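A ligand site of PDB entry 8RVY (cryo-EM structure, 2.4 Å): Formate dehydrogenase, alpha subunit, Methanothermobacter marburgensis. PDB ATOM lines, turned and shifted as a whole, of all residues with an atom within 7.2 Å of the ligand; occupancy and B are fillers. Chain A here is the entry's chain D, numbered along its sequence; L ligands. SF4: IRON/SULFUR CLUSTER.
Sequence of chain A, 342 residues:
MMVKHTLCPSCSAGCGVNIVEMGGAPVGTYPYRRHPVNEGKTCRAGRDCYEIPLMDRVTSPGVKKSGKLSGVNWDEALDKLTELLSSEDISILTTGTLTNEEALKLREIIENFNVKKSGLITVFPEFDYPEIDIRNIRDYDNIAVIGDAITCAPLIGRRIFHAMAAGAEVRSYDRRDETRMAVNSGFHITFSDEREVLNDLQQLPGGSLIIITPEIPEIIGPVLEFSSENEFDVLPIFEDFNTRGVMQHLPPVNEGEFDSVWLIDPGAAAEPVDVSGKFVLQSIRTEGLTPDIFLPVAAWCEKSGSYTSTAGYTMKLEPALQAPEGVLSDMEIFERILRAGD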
ATOM      1  N   LEU A   7       0.750 -30.248   4.839  1.00  0.00           N
ATOM      2  CA  LEU A   7       1.151 -29.187   5.741  1.00  0.00           C
ATOM      3  C   LEU A   7      -0.055 -28.704   6.523  1.00  0.00           C
ATOM      4  O   LEU A   7      -1.140 -28.529   5.959  1.00  0.00           O
ATOM      5  CB  LEU A   7       1.779 -28.023   4.955  1.00  0.00           C
ATOM      6  CG  LEU A   7       2.084 -26.734   5.705  1.00  0.00           C
ATOM      7  CD1 LEU A   7       3.577 -26.617   5.981  1.00  0.00           C
ATOM      8  CD2 LEU A   7       1.600 -25.536   4.910  1.00  0.00           C
ATOM      9  N   CYS A   8       0.131 -28.491   7.812  1.00  0.00           N
ATOM     10  CA  CYS A   8      -0.953 -27.952   8.622  1.00  0.00           C
ATOM     11  C   CYS A   8      -1.220 -26.500   8.215  1.00  0.00           C
ATOM     12  O   CYS A   8      -0.281 -25.688   8.202  1.00  0.00           O
ATOM     13  CB  CYS A   8      -0.615 -28.019  10.095  1.00  0.00           C
ATOM     14  SG  CYS A   8      -1.812 -27.166  11.136  1.00  0.00           S
ATOM     15  N   PRO A   9      -2.456 -26.136   7.885  1.00  0.00           N
ATOM     16  CA  PRO A   9      -2.747 -24.756   7.456  1.00  0.00           C
ATOM     17  C   PRO A   9      -3.245 -23.820   8.554  1.00  0.00           C
ATOM     18  O   PRO A   9      -3.625 -22.697   8.230  1.00  0.00           O
ATOM     19  CB  PRO A   9      -3.852 -24.988   6.414  1.00  0.00           C
ATOM     20  CG  PRO A   9      -4.622 -26.139   6.976  1.00  0.00           C
ATOM     21  CD  PRO A   9      -3.655 -26.987   7.769  1.00  0.00           C
ATOM     22  N   SER A  10      -3.230 -24.243   9.811  1.00  0.00           N
ATOM     23  CA  SER A  10      -3.912 -23.506  10.866  1.00  0.00           C
ATOM     24  C   SER A  10      -3.095 -22.344  11.421  1.00  0.00           C
ATOM     25  O   SER A  10      -3.652 -21.506  12.135  1.00  0.00           O
ATOM     26  CB  SER A  10      -4.297 -24.459  11.995  1.00  0.00           C
ATOM     27  OG  SER A  10      -5.277 -25.376  11.551  1.00  0.00           O
ATOM     28  N   CYS A  11      -1.798 -22.280  11.137  1.00  0.00           N
ATOM     29  CA  CYS A  11      -1.041 -21.053  11.399  1.00  0.00           C
ATOM     30  C   CYS A  11       0.207 -21.091  10.521  1.00  0.00           C
ATOM     31  O   CYS A  11       0.408 -22.004   9.719  1.00  0.00           O
ATOM     32  CB  CYS A  11      -0.673 -20.904  12.875  1.00  0.00           C
ATOM     33  SG  CYS A  11       0.708 -21.892  13.437  1.00  0.00           S
ATOM     34  N   SER A  12       1.049 -20.074  10.695  1.00  0.00           N
ATOM     35  CA  SER A  12       2.181 -19.870   9.800  1.00  0.00           C
ATOM     36  C   SER A  12       3.292 -20.880  10.015  1.00  0.00           C
ATOM     37  O   SER A  12       4.067 -21.124   9.088  1.00  0.00           O
ATOM     38  CB  SER A  12       2.708 -18.452   9.952  1.00  0.00           C
ATOM     39  OG  SER A  12       2.916 -18.143  11.316  1.00  0.00           O
ATOM     40  N   ALA A  13       3.399 -21.486  11.196  1.00  0.00           N
ATOM     41  CA  ALA A  13       4.422 -22.498  11.419  1.00  0.00           C
ATOM     42  C   ALA A  13       4.234 -23.634  10.421  1.00  0.00           C
ATOM     43  O   ALA A  13       3.106 -24.028  10.110  1.00  0.00           O
ATOM     44  CB  ALA A  13       4.352 -23.027  12.849  1.00  0.00           C
ATOM     45  N   GLY A  14       5.346 -24.151   9.908  1.00  0.00           N
ATOM     46  CA  GLY A  14       5.262 -25.077   8.801  1.00  0.00           C
ATOM     47  C   GLY A  14       5.083 -26.530   9.181  1.00  0.00           C
ATOM     48  O   GLY A  14       5.616 -27.409   8.502  1.00  0.00           O
ATOM     49  N   CYS A  15       4.320 -26.792  10.233  1.00  0.00           N
ATOM     50  CA  CYS A  15       4.196 -28.157  10.741  1.00  0.00           C
ATOM     51  C   CYS A  15       3.642 -29.094   9.674  1.00  0.00           C
ATOM     52  O   CYS A  15       2.730 -28.741   8.925  1.00  0.00           O
ATOM     53  CB  CYS A  15       3.307 -28.181  11.972  1.00  0.00           C
ATOM     54  SG  CYS A  15       3.920 -27.208  13.359  1.00  0.00           S
ATOM     55  N   GLY A  16       4.203 -30.300   9.605  1.00  0.00           N
ATOM     56  CA  GLY A  16       3.712 -31.331   8.717  1.00  0.00           C
ATOM     57  C   GLY A  16       2.806 -32.319   9.431  1.00  0.00           C
ATOM     58  O   GLY A  16       2.967 -32.583  10.616  1.00  0.00           O
ATOM     59  N   VAL A  17       1.826 -32.842   8.697  1.00  0.00           N
ATOM     60  CA  VAL A  17       0.872 -33.798   9.237  1.00  0.00           C
ATOM     61  C   VAL A  17       0.526 -34.789   8.136  1.00  0.00           C
ATOM     62  O   VAL A  17       0.549 -34.457   6.960  1.00  0.00           O
ATOM     63  CB  VAL A  17      -0.406 -33.108   9.768  1.00  0.00           C
ATOM     64  CG1 VAL A  17      -0.110 -32.341  11.031  1.00  0.00           C
ATOM     65  CG2 VAL A  17      -0.980 -32.169   8.720  1.00  0.00           C
ATOM     66  N   VAL A  37      10.228 -29.367  10.995  1.00  0.00           N
ATOM     67  CA  VAL A  37       9.710 -28.232  11.750  1.00  0.00           C
ATOM     68  C   VAL A  37       9.196 -28.684  13.103  1.00  0.00           C
ATOM     69  O   VAL A  37       9.534 -28.100  14.139  1.00  0.00           O
ATOM     70  CB  VAL A  37       8.608 -27.507  10.939  1.00  0.00           C
ATOM     71  CG1 VAL A  37       7.822 -26.570  11.830  1.00  0.00           C
ATOM     72  CG2 VAL A  37       9.224 -26.745   9.789  1.00  0.00           C
ATOM     73  N   ASN A  38       8.370 -29.731  13.122  1.00  0.00           N
ATOM     74  CA  ASN A  38       7.709 -30.164  14.345  1.00  0.00           C
ATOM     75  C   ASN A  38       8.018 -31.598  14.758  1.00  0.00           C
ATOM     76  O   ASN A  38       7.853 -31.923  15.934  1.00  0.00           O
ATOM     77  CB  ASN A  38       6.191 -30.027  14.204  1.00  0.00           C
ATOM     78  CG  ASN A  38       5.629 -30.813  13.052  1.00  0.00           C
ATOM     79  OD1 ASN A  38       6.245 -30.912  11.996  1.00  0.00           O
ATOM     80  ND2 ASN A  38       4.452 -31.390  13.249  1.00  0.00           N
ATOM     81  N   LYS A  41       4.930 -33.467  16.088  1.00  0.00           N
ATOM     82  CA  LYS A  41       4.195 -32.808  17.149  1.00  0.00           C
ATOM     83  C   LYS A  41       3.254 -31.761  16.556  1.00  0.00           C
ATOM     84  O   LYS A  41       3.615 -31.060  15.607  1.00  0.00           O
ATOM     85  CB  LYS A  41       5.152 -32.155  18.143  1.00  0.00           C
ATOM     86  CG  LYS A  41       6.123 -33.126  18.775  1.00  0.00           C
ATOM     87  CD  LYS A  41       7.337 -32.436  19.335  1.00  0.00           C
ATOM     88  CE  LYS A  41       8.361 -33.423  19.839  1.00  0.00           C
ATOM     89  NZ  LYS A  41       7.955 -34.035  21.130  1.00  0.00           N
ATOM     90  N   THR A  42       2.047 -31.691  17.096  1.00  0.00           N
ATOM     91  CA  THR A  42       1.066 -30.724  16.636  1.00  0.00           C
ATOM     92  C   THR A  42       0.235 -30.248  17.819  1.00  0.00           C
ATOM     93  O   THR A  42       0.077 -30.959  18.814  1.00  0.00           O
ATOM     94  CB  THR A  42       0.138 -31.294  15.562  1.00  0.00           C
ATOM     95  OG1 THR A  42      -0.453 -32.513  16.034  1.00  0.00           O
ATOM     96  CG2 THR A  42       0.881 -31.570  14.285  1.00  0.00           C
ATOM     97  N   CYS A  43      -0.300 -29.032  17.691  1.00  0.00           N
ATOM     98  CA  CYS A  43      -1.295 -28.538  18.625  1.00  0.00           C
ATOM     99  C   CYS A  43      -2.665 -29.065  18.231  1.00  0.00           C
ATOM    100  O   CYS A  43      -2.817 -29.789  17.245  1.00  0.00           O
ATOM    101  CB  CYS A  43      -1.258 -27.016  18.669  1.00  0.00           C
ATOM    102  SG  CYS A  43      -1.882 -26.218  17.171  1.00  0.00           S
ATOM    103  N   ARG A  44      -3.688 -28.693  18.997  1.00  0.00           N
ATOM    104  CA  ARG A  44      -5.035 -29.178  18.699  1.00  0.00           C
ATOM    105  C   ARG A  44      -5.455 -28.769  17.291  1.00  0.00           C
ATOM    106  O   ARG A  44      -6.131 -29.526  16.593  1.00  0.00           O
ATOM    107  CB  ARG A  44      -6.022 -28.665  19.739  1.00  0.00           C
ATOM    108  CG  ARG A  44      -7.402 -29.296  19.645  1.00  0.00           C
ATOM    109  CD  ARG A  44      -7.393 -30.733  20.129  1.00  0.00           C
ATOM    110  NE  ARG A  44      -8.599 -31.096  20.866  1.00  0.00           N
ATOM    111  CZ  ARG A  44      -8.968 -30.567  22.016  1.00  0.00           C
ATOM    112  NH1 ARG A  44      -8.260 -29.609  22.596  1.00  0.00           N
ATOM    113  NH2 ARG A  44     -10.080 -30.996  22.613  1.00  0.00           N
ATOM    114  N   ALA A  45      -5.071 -27.565  16.860  1.00  0.00           N
ATOM    115  CA  ALA A  45      -5.454 -27.092  15.540  1.00  0.00           C
ATOM    116  C   ALA A  45      -4.873 -27.975  14.446  1.00  0.00           C
ATOM    117  O   ALA A  45      -5.510 -28.189  13.401  1.00  0.00           O
ATOM    118  CB  ALA A  45      -5.017 -25.647  15.347  1.00  0.00           C
ATOM    119  N   GLY A  46      -3.662 -28.490  14.649  1.00  0.00           N
ATOM    120  CA  GLY A  46      -3.036 -29.337  13.652  1.00  0.00           C
ATOM    121  C   GLY A  46      -3.644 -30.713  13.535  1.00  0.00           C
ATOM    122  O   GLY A  46      -3.528 -31.348  12.481  1.00  0.00           O
ATOM    123  N   ARG A  47      -4.283 -31.207  14.599  1.00  0.00           N
ATOM    124  CA  ARG A  47      -4.882 -32.524  14.574  1.00  0.00           C
ATOM    125  C   ARG A  47      -6.344 -32.510  14.160  1.00  0.00           C
ATOM    126  O   ARG A  47      -6.938 -33.571  13.979  1.00  0.00           O
ATOM    127  CB  ARG A  47      -4.748 -33.187  15.947  1.00  0.00           C
ATOM    128  CG  ARG A  47      -3.544 -34.118  16.047  1.00  0.00           C
ATOM    129  CD  ARG A  47      -3.190 -34.433  17.488  1.00  0.00           C
ATOM    130  NE  ARG A  47      -2.748 -33.253  18.219  1.00  0.00           N
ATOM    131  CZ  ARG A  47      -3.393 -32.686  19.226  1.00  0.00           C
ATOM    132  NH1 ARG A  47      -4.561 -33.149  19.649  1.00  0.00           N
ATOM    133  NH2 ARG A  47      -2.868 -31.617  19.822  1.00  0.00           N
ATOM    134  N   CYS A  49      -7.217 -30.488  11.417  1.00  0.00           N
ATOM    135  CA  CYS A  49      -7.198 -29.895  10.082  1.00  0.00           C
ATOM    136  C   CYS A  49      -7.824 -30.795   9.028  1.00  0.00           C
ATOM    137  O   CYS A  49      -8.296 -30.291   8.009  1.00  0.00           O
ATOM    138  CB  CYS A  49      -5.768 -29.531   9.693  1.00  0.00           C
ATOM    139  SG  CYS A  49      -4.705 -30.938   9.321  1.00  0.00           S
ATOM    140  N   ILE A 150       3.933 -18.330  22.043  1.00  0.00           N
ATOM    141  CA  ILE A 150       3.546 -19.706  22.356  1.00  0.00           C
ATOM    142  C   ILE A 150       2.129 -19.982  21.880  1.00  0.00           C
ATOM    143  O   ILE A 150       1.841 -21.053  21.318  1.00  0.00           O
ATOM    144  CB  ILE A 150       3.699 -19.979  23.855  1.00  0.00           C
ATOM    145  CG1 ILE A 150       5.174 -19.979  24.256  1.00  0.00           C
ATOM    146  CG2 ILE A 150       3.061 -21.313  24.208  1.00  0.00           C
ATOM    147  CD1 ILE A 150       5.410 -19.944  25.743  1.00  0.00           C
ATOM    148  N   THR A 151       1.215 -19.044  22.097  1.00  0.00           N
ATOM    149  CA  THR A 151      -0.173 -19.276  21.710  1.00  0.00           C
ATOM    150  C   THR A 151      -0.376 -19.134  20.206  1.00  0.00           C
ATOM    151  O   THR A 151      -1.164 -19.872  19.613  1.00  0.00           O
ATOM    152  CB  THR A 151      -1.103 -18.327  22.457  1.00  0.00           C
ATOM    153  OG1 THR A 151      -1.088 -18.640  23.852  1.00  0.00           O
ATOM    154  CG2 THR A 151      -2.530 -18.430  21.926  1.00  0.00           C
ATOM    155  N   CYS A 152       0.313 -18.189  19.577  1.00  0.00           N
ATOM    156  CA  CYS A 152       0.137 -17.972  18.145  1.00  0.00           C
ATOM    157  C   CYS A 152       0.609 -19.190  17.352  1.00  0.00           C
ATOM    158  O   CYS A 152      -0.134 -19.714  16.520  1.00  0.00           O
ATOM    159  CB  CYS A 152       0.893 -16.725  17.708  1.00  0.00           C
ATOM    160  SG  CYS A 152       0.112 -15.175  18.191  1.00  0.00           S
ATOM    161  N   ALA A 153       1.829 -19.639  17.602  1.00  0.00           N
ATOM    162  CA  ALA A 153       2.379 -20.844  16.990  1.00  0.00           C
ATOM    163  C   ALA A 153       3.034 -21.676  18.079  1.00  0.00           C
ATOM    164  O   ALA A 153       4.199 -21.444  18.429  1.00  0.00           O
ATOM    165  CB  ALA A 153       3.376 -20.500  15.884  1.00  0.00           C
ATOM    166  N   PRO A 154       2.312 -22.651  18.644  1.00  0.00           N
ATOM    167  CA  PRO A 154       2.899 -23.445  19.739  1.00  0.00           C
ATOM    168  C   PRO A 154       4.223 -24.106  19.398  1.00  0.00           C
ATOM    169  O   PRO A 154       5.094 -24.229  20.266  1.00  0.00           O
ATOM    170  CB  PRO A 154       1.809 -24.486  20.019  1.00  0.00           C
ATOM    171  CG  PRO A 154       0.554 -23.852  19.595  1.00  0.00           C
ATOM    172  CD  PRO A 154       0.871 -22.899  18.484  1.00  0.00           C
ATOM    173  N   LEU A 155       4.405 -24.541  18.150  1.00  0.00           N
ATOM    174  CA  LEU A 155       5.598 -25.307  17.798  1.00  0.00           C
ATOM    175  C   LEU A 155       6.829 -24.442  17.603  1.00  0.00           C
ATOM    176  O   LEU A 155       7.925 -24.987  17.479  1.00  0.00           O
ATOM    177  CB  LEU A 155       5.322 -26.143  16.553  1.00  0.00           C
ATOM    178  CG  LEU A 155       4.814 -27.565  16.817  1.00  0.00           C
ATOM    179  CD1 LEU A 155       5.823 -28.364  17.624  1.00  0.00           C
ATOM    180  CD2 LEU A 155       3.465 -27.559  17.519  1.00  0.00           C
ATOM    181  N   ILE A 156       6.690 -23.124  17.582  1.00  0.00           N
ATOM    182  CA  ILE A 156       7.851 -22.243  17.707  1.00  0.00           C
ATOM    183  C   ILE A 156       8.097 -21.870  19.159  1.00  0.00           C
ATOM    184  O   ILE A 156       9.249 -21.659  19.566  1.00  0.00           O
ATOM    185  CB  ILE A 156       7.661 -20.990  16.828  1.00  0.00           C
ATOM    186  CG1 ILE A 156       7.767 -21.360  15.348  1.00  0.00           C
ATOM    187  CG2 ILE A 156       8.718 -19.945  17.161  1.00  0.00           C
ATOM    188  CD1 ILE A 156       6.793 -20.631  14.472  1.00  0.00           C
ATOM    189  N   PHE A 241      -0.876 -19.594   6.631  1.00  0.00           N
ATOM    190  CA  PHE A 241       0.180 -20.592   6.566  1.00  0.00           C
ATOM    191  C   PHE A 241       1.194 -20.271   5.477  1.00  0.00           C
ATOM    192  O   PHE A 241       2.395 -20.527   5.659  1.00  0.00           O
ATOM    193  CB  PHE A 241      -0.394 -21.992   6.379  1.00  0.00           C
ATOM    194  CG  PHE A 241      -1.195 -22.173   5.126  1.00  0.00           C
ATOM    195  CD1 PHE A 241      -2.545 -21.882   5.091  1.00  0.00           C
ATOM    196  CD2 PHE A 241      -0.607 -22.680   3.992  1.00  0.00           C
ATOM    197  CE1 PHE A 241      -3.280 -22.071   3.946  1.00  0.00           C
ATOM    198  CE2 PHE A 241      -1.338 -22.867   2.839  1.00  0.00           C
ATOM    199  CZ  PHE A 241      -2.679 -22.565   2.824  1.00  0.00           C
HETATM  200 FE1  SF4 L   1       1.842 -26.429  13.890  1.00  0.00          FE
HETATM  201 FE2  SF4 L   1      -0.265 -26.030  15.582  1.00  0.00          FE
HETATM  202 FE3  SF4 L   1      -0.696 -26.290  12.892  1.00  0.00          FE
HETATM  203 FE4  SF4 L   1       0.514 -24.049  13.872  1.00  0.00          FE
HETATM  204  S1  SF4 L   1      -1.623 -24.740  14.278  1.00  0.00           S
HETATM  205  S2  SF4 L   1       1.152 -25.266  12.056  1.00  0.00           S
HETATM  206  S3  SF4 L   1       1.722 -24.924  15.590  1.00  0.00           S
HETATM  207  S4  SF4 L   1       0.128 -27.875  14.313  1.00  0.00           S
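O of Ala 13 sits close to S2 of the ligand, 3.0 Å away.
Ser 10 touches the ligand.
Thr 42 touches the ligand.
Ala 45 touches the ligand (CB to S1, 3.7 Å).
CA of Gly 46 touches S4 of the ligand (3.5 Å).
Pro 154 touches the ligand (CD to S3, 3.6 Å).
Of the 29 residues printed, 11 come within 4 Å of the ligand.
The nearest printed residue that does not touch the ligand is Ala 153 (4.3 Å).
SG of Cys 11 sits close to N of Ala 13 (3.5 Å).
The backbone carbonyl oxygen (O) of Cys 15 sits at hydrogen-bond distance from the backbone NH (N) of Cys 8.
The side-chain sulfur of Cys 8 sits close to the backbone NH of Ser 10.
The backbone NH of Ala 45 lies close to the side-chain sulfur of Cys 43.
The backbone carbonyl oxygen of Cys 43 lies close to the guanidinium group of Arg 47.
O of Ala 45 lies within hydrogen-bond range of OG of Ser 10.
The backbone carbonyl oxygen (O) of Gly 46 sits at hydrogen-bond distance from the side-chain sulfur (SG) of Cys 49 (3.4 Å).
The backbone carbonyl oxygen (O) of Thr 42 lies within hydrogen-bond range of the guanidinium group (NH2) of Arg 47 (3.2 Å).
An iron atom (FE4) of the ligand is bound by the side-chain sulfur (SG) of Cys 11 (2.2 Å).
SG of Cys 8 binds FE3 of the ligand, 2.3 Å away.
N of Cys 43 sits close to S4 of the ligand (3.6 Å).
The side-chain sulfur of Cys 43 is bound to an iron atom (FE2) of the ligand, at 2.3 Å.
An iron atom (FE1) of the ligand is bound by the side-chain sulfur (SG) of Cys 15, at 2.3 Å.
The backbone NH (N) of Leu 155 sits close to a sulfur (S3) of the ligand (3.7 Å).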
